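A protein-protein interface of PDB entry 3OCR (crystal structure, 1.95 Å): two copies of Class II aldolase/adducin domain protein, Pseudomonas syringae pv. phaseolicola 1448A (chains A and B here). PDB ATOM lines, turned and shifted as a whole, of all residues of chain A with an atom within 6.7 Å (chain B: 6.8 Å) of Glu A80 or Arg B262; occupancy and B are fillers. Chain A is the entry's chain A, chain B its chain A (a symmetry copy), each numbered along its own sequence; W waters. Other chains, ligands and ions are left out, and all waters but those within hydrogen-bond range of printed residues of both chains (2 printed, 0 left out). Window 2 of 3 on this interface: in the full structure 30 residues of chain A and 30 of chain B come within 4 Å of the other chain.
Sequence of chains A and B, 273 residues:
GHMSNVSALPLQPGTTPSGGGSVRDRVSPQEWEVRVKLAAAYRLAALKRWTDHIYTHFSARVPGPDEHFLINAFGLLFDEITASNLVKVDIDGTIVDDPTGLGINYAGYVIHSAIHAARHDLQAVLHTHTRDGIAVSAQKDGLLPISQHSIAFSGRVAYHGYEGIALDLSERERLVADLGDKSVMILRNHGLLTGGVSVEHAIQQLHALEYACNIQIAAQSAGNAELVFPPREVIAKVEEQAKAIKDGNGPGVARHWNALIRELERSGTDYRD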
ATOM      1  N   ARG A  43      26.449 -23.338  -4.798  1.00  0.00           N
ATOM      2  CA  ARG A  43      27.679 -22.560  -4.730  1.00  0.00           C
ATOM      3  C   ARG A  43      28.765 -23.077  -3.800  1.00  0.00           C
ATOM      4  O   ARG A  43      29.953 -22.913  -4.089  1.00  0.00           O
ATOM      5  CB  ARG A  43      27.360 -21.109  -4.314  1.00  0.00           C
ATOM      6  CG  ARG A  43      26.325 -20.462  -5.201  1.00  0.00           C
ATOM      7  CD  ARG A  43      26.958 -19.878  -6.448  1.00  0.00           C
ATOM      8  NE  ARG A  43      26.025 -19.003  -7.150  1.00  0.00           N
ATOM      9  CZ  ARG A  43      26.270 -17.744  -7.502  1.00  0.00           C
ATOM     10  NH1 ARG A  43      27.442 -17.178  -7.261  1.00  0.00           N
ATOM     11  NH2 ARG A  43      25.338 -17.066  -8.139  1.00  0.00           N
ATOM     12  N   ALA A  46      30.449 -25.901  -5.489  1.00  0.00           N
ATOM     13  CA  ALA A  46      31.343 -25.343  -6.484  1.00  0.00           C
ATOM     14  C   ALA A  46      32.620 -24.877  -5.811  1.00  0.00           C
ATOM     15  O   ALA A  46      33.708 -25.223  -6.260  1.00  0.00           O
ATOM     16  CB  ALA A  46      30.654 -24.194  -7.262  1.00  0.00           C
ATOM     17  N   ILE A  54      28.215 -29.665 -15.723  1.00  0.00           N
ATOM     18  CA  ILE A  54      26.783 -29.387 -15.646  1.00  0.00           C
ATOM     19  C   ILE A  54      25.937 -30.579 -15.213  1.00  0.00           C
ATOM     20  O   ILE A  54      24.709 -30.526 -15.303  1.00  0.00           O
ATOM     21  CB  ILE A  54      26.228 -28.816 -16.972  1.00  0.00           C
ATOM     22  CG1 ILE A  54      26.651 -29.684 -18.154  1.00  0.00           C
ATOM     23  CG2 ILE A  54      26.677 -27.371 -17.153  1.00  0.00           C
ATOM     24  CD1 ILE A  54      25.796 -29.513 -19.388  1.00  0.00           C
ATOM     25  N   PHE A  74      18.555 -26.565 -16.496  1.00  0.00           N
ATOM     26  CA  PHE A  74      19.309 -27.390 -17.450  1.00  0.00           C
ATOM     27  C   PHE A  74      20.473 -26.631 -18.057  1.00  0.00           C
ATOM     28  O   PHE A  74      20.269 -25.656 -18.781  1.00  0.00           O
ATOM     29  CB  PHE A  74      18.366 -27.788 -18.593  1.00  0.00           C
ATOM     30  CG  PHE A  74      18.780 -29.036 -19.357  1.00  0.00           C
ATOM     31  CD1 PHE A  74      19.763 -29.896 -18.864  1.00  0.00           C
ATOM     32  CD2 PHE A  74      18.130 -29.371 -20.552  1.00  0.00           C
ATOM     33  CE1 PHE A  74      20.115 -31.070 -19.562  1.00  0.00           C
ATOM     34  CE2 PHE A  74      18.459 -30.538 -21.252  1.00  0.00           C
ATOM     35  CZ  PHE A  74      19.455 -31.386 -20.756  1.00  0.00           C
ATOM     36  N   GLY A  75      21.692 -27.044 -17.740  1.00  0.00           N
ATOM     37  CA  GLY A  75      22.862 -26.446 -18.397  1.00  0.00           C
ATOM     38  C   GLY A  75      23.588 -25.330 -17.659  1.00  0.00           C
ATOM     39  O   GLY A  75      24.627 -24.877 -18.118  1.00  0.00           O
ATOM     40  N   LEU A  76      23.065 -24.896 -16.516  1.00  0.00           N
ATOM     41  CA  LEU A  76      23.783 -23.935 -15.673  1.00  0.00           C
ATOM     42  C   LEU A  76      24.801 -24.638 -14.796  1.00  0.00           C
ATOM     43  O   LEU A  76      24.551 -25.732 -14.323  1.00  0.00           O
ATOM     44  CB  LEU A  76      22.823 -23.179 -14.761  1.00  0.00           C
ATOM     45  CG  LEU A  76      21.866 -22.167 -15.388  1.00  0.00           C
ATOM     46  CD1 LEU A  76      21.312 -21.255 -14.268  1.00  0.00           C
ATOM     47  CD2 LEU A  76      22.552 -21.356 -16.464  1.00  0.00           C
ATOM     48  N   LEU A  77      25.931 -23.984 -14.568  1.00  0.00           N
ATOM     49  CA  LEU A  77      26.934 -24.445 -13.616  1.00  0.00           C
ATOM     50  C   LEU A  77      26.514 -24.136 -12.167  1.00  0.00           C
ATOM     51  O   LEU A  77      25.795 -23.175 -11.922  1.00  0.00           O
ATOM     52  CB  LEU A  77      28.271 -23.767 -13.919  1.00  0.00           C
ATOM     53  CG  LEU A  77      28.882 -24.043 -15.290  1.00  0.00           C
ATOM     54  CD1 LEU A  77      30.096 -23.154 -15.510  1.00  0.00           C
ATOM     55  CD2 LEU A  77      29.262 -25.530 -15.372  1.00  0.00           C
ATOM     56  N   PHE A  78      26.983 -24.953 -11.224  1.00  0.00           N
ATOM     57  CA  PHE A  78      26.682 -24.810  -9.793  1.00  0.00           C
ATOM     58  C   PHE A  78      27.018 -23.405  -9.336  1.00  0.00           C
ATOM     59  O   PHE A  78      26.351 -22.844  -8.471  1.00  0.00           O
ATOM     60  CB  PHE A  78      27.484 -25.829  -8.991  1.00  0.00           C
ATOM     61  CG  PHE A  78      26.847 -27.207  -8.938  1.00  0.00           C
ATOM     62  CD1 PHE A  78      26.043 -27.666  -9.990  1.00  0.00           C
ATOM     63  CD2 PHE A  78      27.041 -28.027  -7.843  1.00  0.00           C
ATOM     64  CE1 PHE A  78      25.449 -28.937  -9.949  1.00  0.00           C
ATOM     65  CE2 PHE A  78      26.457 -29.318  -7.783  1.00  0.00           C
ATOM     66  CZ  PHE A  78      25.660 -29.765  -8.845  1.00  0.00           C
ATOM     67  N   ASP A  79      28.050 -22.859  -9.974  1.00  0.00           N
ATOM     68  CA  ASP A  79      28.592 -21.529  -9.773  1.00  0.00           C
ATOM     69  C   ASP A  79      27.648 -20.403 -10.166  1.00  0.00           C
ATOM     70  O   ASP A  79      27.900 -19.239  -9.861  1.00  0.00           O
ATOM     71  CB  ASP A  79      29.806 -21.408 -10.696  1.00  0.00           C
ATOM     72  CG  ASP A  79      31.034 -20.980  -9.970  1.00  0.00           C
ATOM     73  OD1 ASP A  79      30.920 -20.636  -8.774  1.00  0.00           O
ATOM     74  OD2 ASP A  79      32.119 -20.990 -10.581  1.00  0.00           O
ATOM     75  N   GLU A  80      26.600 -20.742 -10.902  1.00  0.00           N
ATOM     76  CA  GLU A  80      25.730 -19.737 -11.493  1.00  0.00           C
ATOM     77  C   GLU A  80      24.390 -19.734 -10.797  1.00  0.00           C
ATOM     78  O   GLU A  80      23.558 -18.864 -11.033  1.00  0.00           O
ATOM     79  CB  GLU A  80      25.531 -20.004 -12.989  1.00  0.00           C
ATOM     80  CG  GLU A  80      26.776 -19.788 -13.842  1.00  0.00           C
ATOM     81  CD  GLU A  80      26.570 -20.234 -15.287  1.00  0.00           C
ATOM     82  OE1 GLU A  80      26.078 -21.364 -15.526  1.00  0.00           O
ATOM     83  OE2 GLU A  80      26.921 -19.454 -16.184  1.00  0.00           O
ATOM     84  N   ILE A  81      24.181 -20.711  -9.926  1.00  0.00           N
ATOM     85  CA  ILE A  81      22.862 -20.915  -9.346  1.00  0.00           C
ATOM     86  C   ILE A  81      22.553 -19.786  -8.359  1.00  0.00           C
ATOM     87  O   ILE A  81      23.440 -19.349  -7.614  1.00  0.00           O
ATOM     88  CB  ILE A  81      22.759 -22.267  -8.663  1.00  0.00           C
ATOM     89  CG1 ILE A  81      23.171 -23.403  -9.639  1.00  0.00           C
ATOM     90  CG2 ILE A  81      21.345 -22.474  -8.056  1.00  0.00           C
ATOM     91  CD1 ILE A  81      22.391 -23.458 -10.985  1.00  0.00           C
ATOM     92  N   THR A  82      21.312 -19.315  -8.383  1.00  0.00           N
ATOM     93  CA  THR A  82      20.845 -18.286  -7.457  1.00  0.00           C
ATOM     94  C   THR A  82      19.464 -18.681  -6.932  1.00  0.00           C
ATOM     95  O   THR A  82      18.760 -19.466  -7.557  1.00  0.00           O
ATOM     96  CB  THR A  82      20.693 -16.912  -8.145  1.00  0.00           C
ATOM     97  OG1 THR A  82      19.630 -16.993  -9.088  1.00  0.00           O
ATOM     98  CG2 THR A  82      21.972 -16.480  -8.870  1.00  0.00           C
ATOM     99  N   ASN A  85      16.949 -18.287  -9.669  1.00  0.00           N
ATOM    100  CA  ASN A  85      16.926 -19.040 -10.934  1.00  0.00           C
ATOM    101  C   ASN A  85      16.714 -20.554 -10.806  1.00  0.00           C
ATOM    102  O   ASN A  85      16.667 -21.292 -11.811  1.00  0.00           O
ATOM    103  CB  ASN A  85      18.093 -18.631 -11.874  1.00  0.00           C
ATOM    104  CG  ASN A  85      19.468 -19.132 -11.422  1.00  0.00           C
ATOM    105  OD1 ASN A  85      19.613 -20.144 -10.709  1.00  0.00           O
ATOM    106  ND2 ASN A  85      20.500 -18.443 -11.895  1.00  0.00           N
ATOM    107  N   LEU A 102      14.897 -22.383 -19.280  1.00  0.00           N
ATOM    108  CA  LEU A 102      15.833 -23.450 -19.676  1.00  0.00           C
ATOM    109  C   LEU A 102      15.328 -24.842 -19.342  1.00  0.00           C
ATOM    110  O   LEU A 102      15.872 -25.835 -19.811  1.00  0.00           O
ATOM    111  CB  LEU A 102      17.211 -23.256 -19.027  1.00  0.00           C
ATOM    112  CG  LEU A 102      18.040 -22.017 -19.383  1.00  0.00           C
ATOM    113  CD1 LEU A 102      19.232 -21.885 -18.438  1.00  0.00           C
ATOM    114  CD2 LEU A 102      18.503 -22.048 -20.838  1.00  0.00           C
ATOM    115  N   ARG B 255      25.332 -27.613 -25.327  1.00  0.00           N
ATOM    116  CA  ARG B 255      25.058 -27.230 -23.940  1.00  0.00           C
ATOM    117  C   ARG B 255      26.333 -27.263 -23.077  1.00  0.00           C
ATOM    118  O   ARG B 255      26.615 -26.328 -22.318  1.00  0.00           O
ATOM    119  CB  ARG B 255      23.976 -28.151 -23.360  1.00  0.00           C
ATOM    120  CG  ARG B 255      23.494 -27.807 -21.971  1.00  0.00           C
ATOM    121  CD  ARG B 255      22.394 -28.770 -21.489  1.00  0.00           C
ATOM    122  NE  ARG B 255      21.257 -28.753 -22.398  1.00  0.00           N
ATOM    123  CZ  ARG B 255      20.923 -29.765 -23.194  1.00  0.00           C
ATOM    124  NH1 ARG B 255      21.602 -30.909 -23.162  1.00  0.00           N
ATOM    125  NH2 ARG B 255      19.881 -29.644 -24.001  1.00  0.00           N
ATOM    126  N   TRP B 257      29.409 -27.166 -24.146  1.00  0.00           N
ATOM    127  CA  TRP B 257      30.358 -26.191 -24.650  1.00  0.00           C
ATOM    128  C   TRP B 257      29.983 -24.777 -24.188  1.00  0.00           C
ATOM    129  O   TRP B 257      30.862 -23.999 -23.795  1.00  0.00           O
ATOM    130  CB  TRP B 257      30.391 -26.218 -26.175  1.00  0.00           C
ATOM    131  CG  TRP B 257      31.207 -25.100 -26.782  1.00  0.00           C
ATOM    132  CD1 TRP B 257      30.745 -23.907 -27.305  1.00  0.00           C
ATOM    133  CD2 TRP B 257      32.632 -25.088 -26.941  1.00  0.00           C
ATOM    134  NE1 TRP B 257      31.810 -23.168 -27.781  1.00  0.00           N
ATOM    135  CE2 TRP B 257      32.976 -23.861 -27.554  1.00  0.00           C
ATOM    136  CE3 TRP B 257      33.648 -25.994 -26.613  1.00  0.00           C
ATOM    137  CZ2 TRP B 257      34.306 -23.521 -27.863  1.00  0.00           C
ATOM    138  CZ3 TRP B 257      34.971 -25.659 -26.901  1.00  0.00           C
ATOM    139  CH2 TRP B 257      35.286 -24.430 -27.521  1.00  0.00           C
ATOM    140  N   ASN B 258      28.697 -24.450 -24.249  1.00  0.00           N
ATOM    141  CA  ASN B 258      28.227 -23.082 -23.919  1.00  0.00           C
ATOM    142  C   ASN B 258      28.510 -22.717 -22.452  1.00  0.00           C
ATOM    143  O   ASN B 258      28.715 -21.542 -22.120  1.00  0.00           O
ATOM    144  CB  ASN B 258      26.721 -22.947 -24.179  1.00  0.00           C
ATOM    145  CG  ASN B 258      26.372 -22.907 -25.655  1.00  0.00           C
ATOM    146  OD1 ASN B 258      27.230 -22.720 -26.512  1.00  0.00           O
ATOM    147  ND2 ASN B 258      25.090 -23.055 -25.955  1.00  0.00           N
ATOM    148  N   ALA B 259      28.479 -23.718 -21.579  1.00  0.00           N
ATOM    149  CA  ALA B 259      28.806 -23.531 -20.159  1.00  0.00           C
ATOM    150  C   ALA B 259      30.312 -23.338 -19.981  1.00  0.00           C
ATOM    151  O   ALA B 259      30.739 -22.468 -19.237  1.00  0.00           O
ATOM    152  CB  ALA B 259      28.301 -24.705 -19.299  1.00  0.00           C
ATOM    153  N   LEU B 260      31.114 -24.144 -20.662  1.00  0.00           N
ATOM    154  CA  LEU B 260      32.569 -23.925 -20.679  1.00  0.00           C
ATOM    155  C   LEU B 260      32.902 -22.489 -21.094  1.00  0.00           C
ATOM    156  O   LEU B 260      33.730 -21.842 -20.461  1.00  0.00           O
ATOM    157  CB  LEU B 260      33.272 -24.924 -21.592  1.00  0.00           C
ATOM    158  CG  LEU B 260      33.313 -26.359 -21.045  1.00  0.00           C
ATOM    159  CD1 LEU B 260      34.052 -27.285 -22.001  1.00  0.00           C
ATOM    160  CD2 LEU B 260      33.948 -26.454 -19.655  1.00  0.00           C
ATOM    161  N   ILE B 261      32.249 -22.005 -22.148  1.00  0.00           N
ATOM    162  CA  ILE B 261      32.430 -20.606 -22.634  1.00  0.00           C
ATOM    163  C   ILE B 261      32.048 -19.555 -21.597  1.00  0.00           C
ATOM    164  O   ILE B 261      32.809 -18.614 -21.375  1.00  0.00           O
ATOM    165  CB  ILE B 261      31.673 -20.342 -23.963  1.00  0.00           C
ATOM    166  CG1 ILE B 261      32.272 -21.168 -25.109  1.00  0.00           C
ATOM    167  CG2 ILE B 261      31.639 -18.824 -24.333  1.00  0.00           C
ATOM    168  CD1 ILE B 261      33.744 -20.912 -25.369  1.00  0.00           C
ATOM    169  N   ARG B 262      30.872 -19.689 -20.986  1.00  0.00           N
ATOM    170  CA  ARG B 262      30.461 -18.776 -19.912  1.00  0.00           C
ATOM    171  C   ARG B 262      31.502 -18.772 -18.782  1.00  0.00           C
ATOM    172  O   ARG B 262      31.833 -17.718 -18.265  1.00  0.00           O
ATOM    173  CB  ARG B 262      29.055 -19.101 -19.347  1.00  0.00           C
ATOM    174  CG  ARG B 262      27.888 -18.936 -20.321  1.00  0.00           C
ATOM    175  CD  ARG B 262      26.498 -18.909 -19.610  1.00  0.00           C
ATOM    176  NE  ARG B 262      26.289 -20.080 -18.760  1.00  0.00           N
ATOM    177  CZ  ARG B 262      25.906 -21.293 -19.180  1.00  0.00           C
ATOM    178  NH1 ARG B 262      25.616 -21.536 -20.461  1.00  0.00           N
ATOM    179  NH2 ARG B 262      25.790 -22.278 -18.295  1.00  0.00           N
ATOM    180  N   GLU B 263      32.007 -19.954 -18.405  1.00  0.00           N
ATOM    181  CA  GLU B 263      33.028 -20.057 -17.359  1.00  0.00           C
ATOM    182  C   GLU B 263      34.326 -19.378 -17.770  1.00  0.00           C
ATOM    183  O   GLU B 263      34.904 -18.605 -16.997  1.00  0.00           O
ATOM    184  CB  GLU B 263      33.328 -21.519 -17.017  1.00  0.00           C
ATOM    185  CG  GLU B 263      34.115 -21.662 -15.713  1.00  0.00           C
ATOM    186  CD  GLU B 263      34.572 -23.084 -15.450  1.00  0.00           C
ATOM    187  OE1 GLU B 263      33.939 -24.037 -15.967  1.00  0.00           O
ATOM    188  OE2 GLU B 263      35.574 -23.241 -14.723  1.00  0.00           O
ATOM    189  N   LEU B 264      34.781 -19.683 -18.986  1.00  0.00           N
ATOM    190  CA  LEU B 264      35.953 -19.037 -19.558  1.00  0.00           C
ATOM    191  C   LEU B 264      35.845 -17.501 -19.539  1.00  0.00           C
ATOM    192  O   LEU B 264      36.746 -16.841 -19.049  1.00  0.00           O
ATOM    193  CB  LEU B 264      36.230 -19.559 -20.982  1.00  0.00           C
ATOM    194  CG  LEU B 264      37.418 -18.934 -21.742  1.00  0.00           C
ATOM    195  CD1 LEU B 264      38.732 -19.077 -20.973  1.00  0.00           C
ATOM    196  CD2 LEU B 264      37.547 -19.511 -23.124  1.00  0.00           C
ATOM    197  N   GLU B 265      34.735 -16.958 -20.038  1.00  0.00           N
ATOM    198  CA  GLU B 265      34.513 -15.504 -20.151  1.00  0.00           C
ATOM    199  C   GLU B 265      34.609 -14.776 -18.807  1.00  0.00           C
ATOM    200  O   GLU B 265      34.850 -13.559 -18.754  1.00  0.00           O
ATOM    201  CB  GLU B 265      33.127 -15.240 -20.747  1.00  0.00           C
ATOM    202  CG  GLU B 265      32.872 -15.926 -22.083  1.00  0.00           C
ATOM    203  CD  GLU B 265      32.787 -14.962 -23.238  1.00  0.00           C
ATOM    204  OE1 GLU B 265      32.304 -13.837 -23.022  1.00  0.00           O
ATOM    205  OE2 GLU B 265      33.196 -15.324 -24.364  1.00  0.00           O
ATOM    206  N   ARG B 266      34.383 -15.536 -17.734  1.00  0.00           N
ATOM    207  CA  ARG B 266      34.587 -15.104 -16.358  1.00  0.00           C
ATOM    208  C   ARG B 266      36.025 -14.630 -16.123  1.00  0.00           C
ATOM    209  O   ARG B 266      36.265 -13.823 -15.234  1.00  0.00           O
ATOM    210  CB  ARG B 266      34.261 -16.267 -15.423  1.00  0.00           C
ATOM    211  CG  ARG B 266      33.547 -15.897 -14.153  1.00  0.00           C
ATOM    212  CD  ARG B 266      32.804 -17.101 -13.583  1.00  0.00           C
ATOM    213  NE  ARG B 266      31.623 -17.419 -14.382  1.00  0.00           N
ATOM    214  CZ  ARG B 266      30.940 -18.557 -14.314  1.00  0.00           C
ATOM    215  NH1 ARG B 266      31.319 -19.521 -13.481  1.00  0.00           N
ATOM    216  NH2 ARG B 266      29.881 -18.734 -15.095  1.00  0.00           N
ATOM    217  N   SER B 267      36.972 -15.130 -16.922  1.00  0.00           N
ATOM    218  CA  SER B 267      38.379 -14.678 -16.869  1.00  0.00           C
ATOM    219  C   SER B 267      38.703 -13.566 -17.876  1.00  0.00           C
ATOM    220  O   SER B 267      39.868 -13.208 -18.046  1.00  0.00           O
ATOM    221  CB  SER B 267      39.346 -15.847 -17.110  1.00  0.00           C
ATOM    222  OG  SER B 267      38.886 -17.054 -16.529  1.00  0.00           O
ATOM    223  N   TYR B 271      40.506 -14.074 -25.464  1.00  0.00           N
ATOM    224  CA  TYR B 271      40.680 -15.239 -26.332  1.00  0.00           C
ATOM    225  C   TYR B 271      40.071 -15.050 -27.722  1.00  0.00           C
ATOM    226  O   TYR B 271      40.537 -15.648 -28.691  1.00  0.00           O
ATOM    227  CB  TYR B 271      40.119 -16.510 -25.679  1.00  0.00           C
ATOM    228  CG  TYR B 271      38.616 -16.606 -25.717  1.00  0.00           C
ATOM    229  CD1 TYR B 271      37.962 -17.167 -26.820  1.00  0.00           C
ATOM    230  CD2 TYR B 271      37.843 -16.133 -24.657  1.00  0.00           C
ATOM    231  CE1 TYR B 271      36.584 -17.245 -26.872  1.00  0.00           C
ATOM    232  CE2 TYR B 271      36.450 -16.210 -24.697  1.00  0.00           C
ATOM    233  CZ  TYR B 271      35.831 -16.756 -25.810  1.00  0.00           C
ATOM    234  OH  TYR B 271      34.459 -16.833 -25.862  1.00  0.00           O
HETATM  235  O   HOH W   1      25.090 -24.290 -20.961  1.00  0.00           O
HETATM  236  O   HOH W   2      20.110 -25.952 -21.830  1.00  0.00           O
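Hydrophobic or aromatic side chains of chain A within 4 Å of the printed part of chain B: Ile A54, Phe A74, Leu A76 and Leu A77. Of the 13 printed residues of chain B, 5 touch a printed residue of chain A. Printed residues of chain B that touch a printed residue of chain A: Arg B255, Ala B259, Arg B262, Glu B263 and Arg B266. Among the printed residues, 12 pairs touch across the chains.
CG of Arg B255 touches CD1 of Ile A54 (3.9 Å). Ala B259 touches Ile A54 (CB to CG2, 3.8 Å). Phe A74 touches Arg B255. Arg B255 touches Gly A75. O of Gly A75 touches CB of Ala B259, at 3.9 Å. Arg B262 touches Leu A76. Ala B259 touches Leu A77. Glu B263 touches Leu A77 (CB to CD1, 3.9 Å).
Water W1 lies within hydrogen-bond range of the guanidinium group (NH1) of Arg B262 (2.8 Å), the backbone carbonyl oxygen (O) of Arg B255 (2.9 Å), the backbone carbonyl oxygen (O) of Gly A75 (2.9 Å) and the backbone NH (N) of Ala B259 (3.5 Å). Water W2 lies within hydrogen-bond range of O of Phe A74 (3.1 Å) and NE of Arg B255 (3.1 Å).
The backbone carbonyl oxygen (O) of Gly A75 sits at hydrogen-bond distance from the guanidinium group (NH2) of Arg B262. OD2 of Asp A79 lies within salt-bridge range of NH1 of Arg B266. The guanidinium group (NE) of Arg B262 lies within salt-bridge range of the side-chain carboxylate (OE2) of Glu A80 (2.7 Å). The side-chain carboxylate of Glu A80 is in salt-bridge range of the guanidinium group of Arg B266, at 3.2 Å.
No position is printed for both chains.
NE of Arg A43 sits close to O of Asp A79. N of Leu A77 sits at hydrogen-bond distance from OE1 of Glu A80, 2.8 Å away. ND2 of Asn A85 lies within hydrogen-bond range of O of Glu A80 (3.2 Å).
Ala A46 touches none of the printed residues of chain B. Printed residues of chain B within 4 Å of Leu A77: Ala B259 and Glu B263. Of chain B, only Arg B262 (2.7 Å) and Arg B266 (3.2 Å) come within 4 Å of Glu A80. Of the printed residues of chain A, Arg B255 touches Ile A54 (3.9 Å), Phe A74 (3.2 Å) and Gly A75 (3.9 Å). Printed residues of chain A within 4 Å of Ala B259: Ile A54, Gly A75 and Leu A77. Arg B262 touches just these residues of chain A: Gly A75 (2.9 Å), Leu A76 (3.7 Å) and Glu A80 (2.7 Å). Of the printed residues of chain A, Arg B266 touches Asp A79 (3.3 Å) and Glu A80 (3.2 Å). The nearest residue of chain B that does not touch Glu A80 is Ala B259 (5.5 Å).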
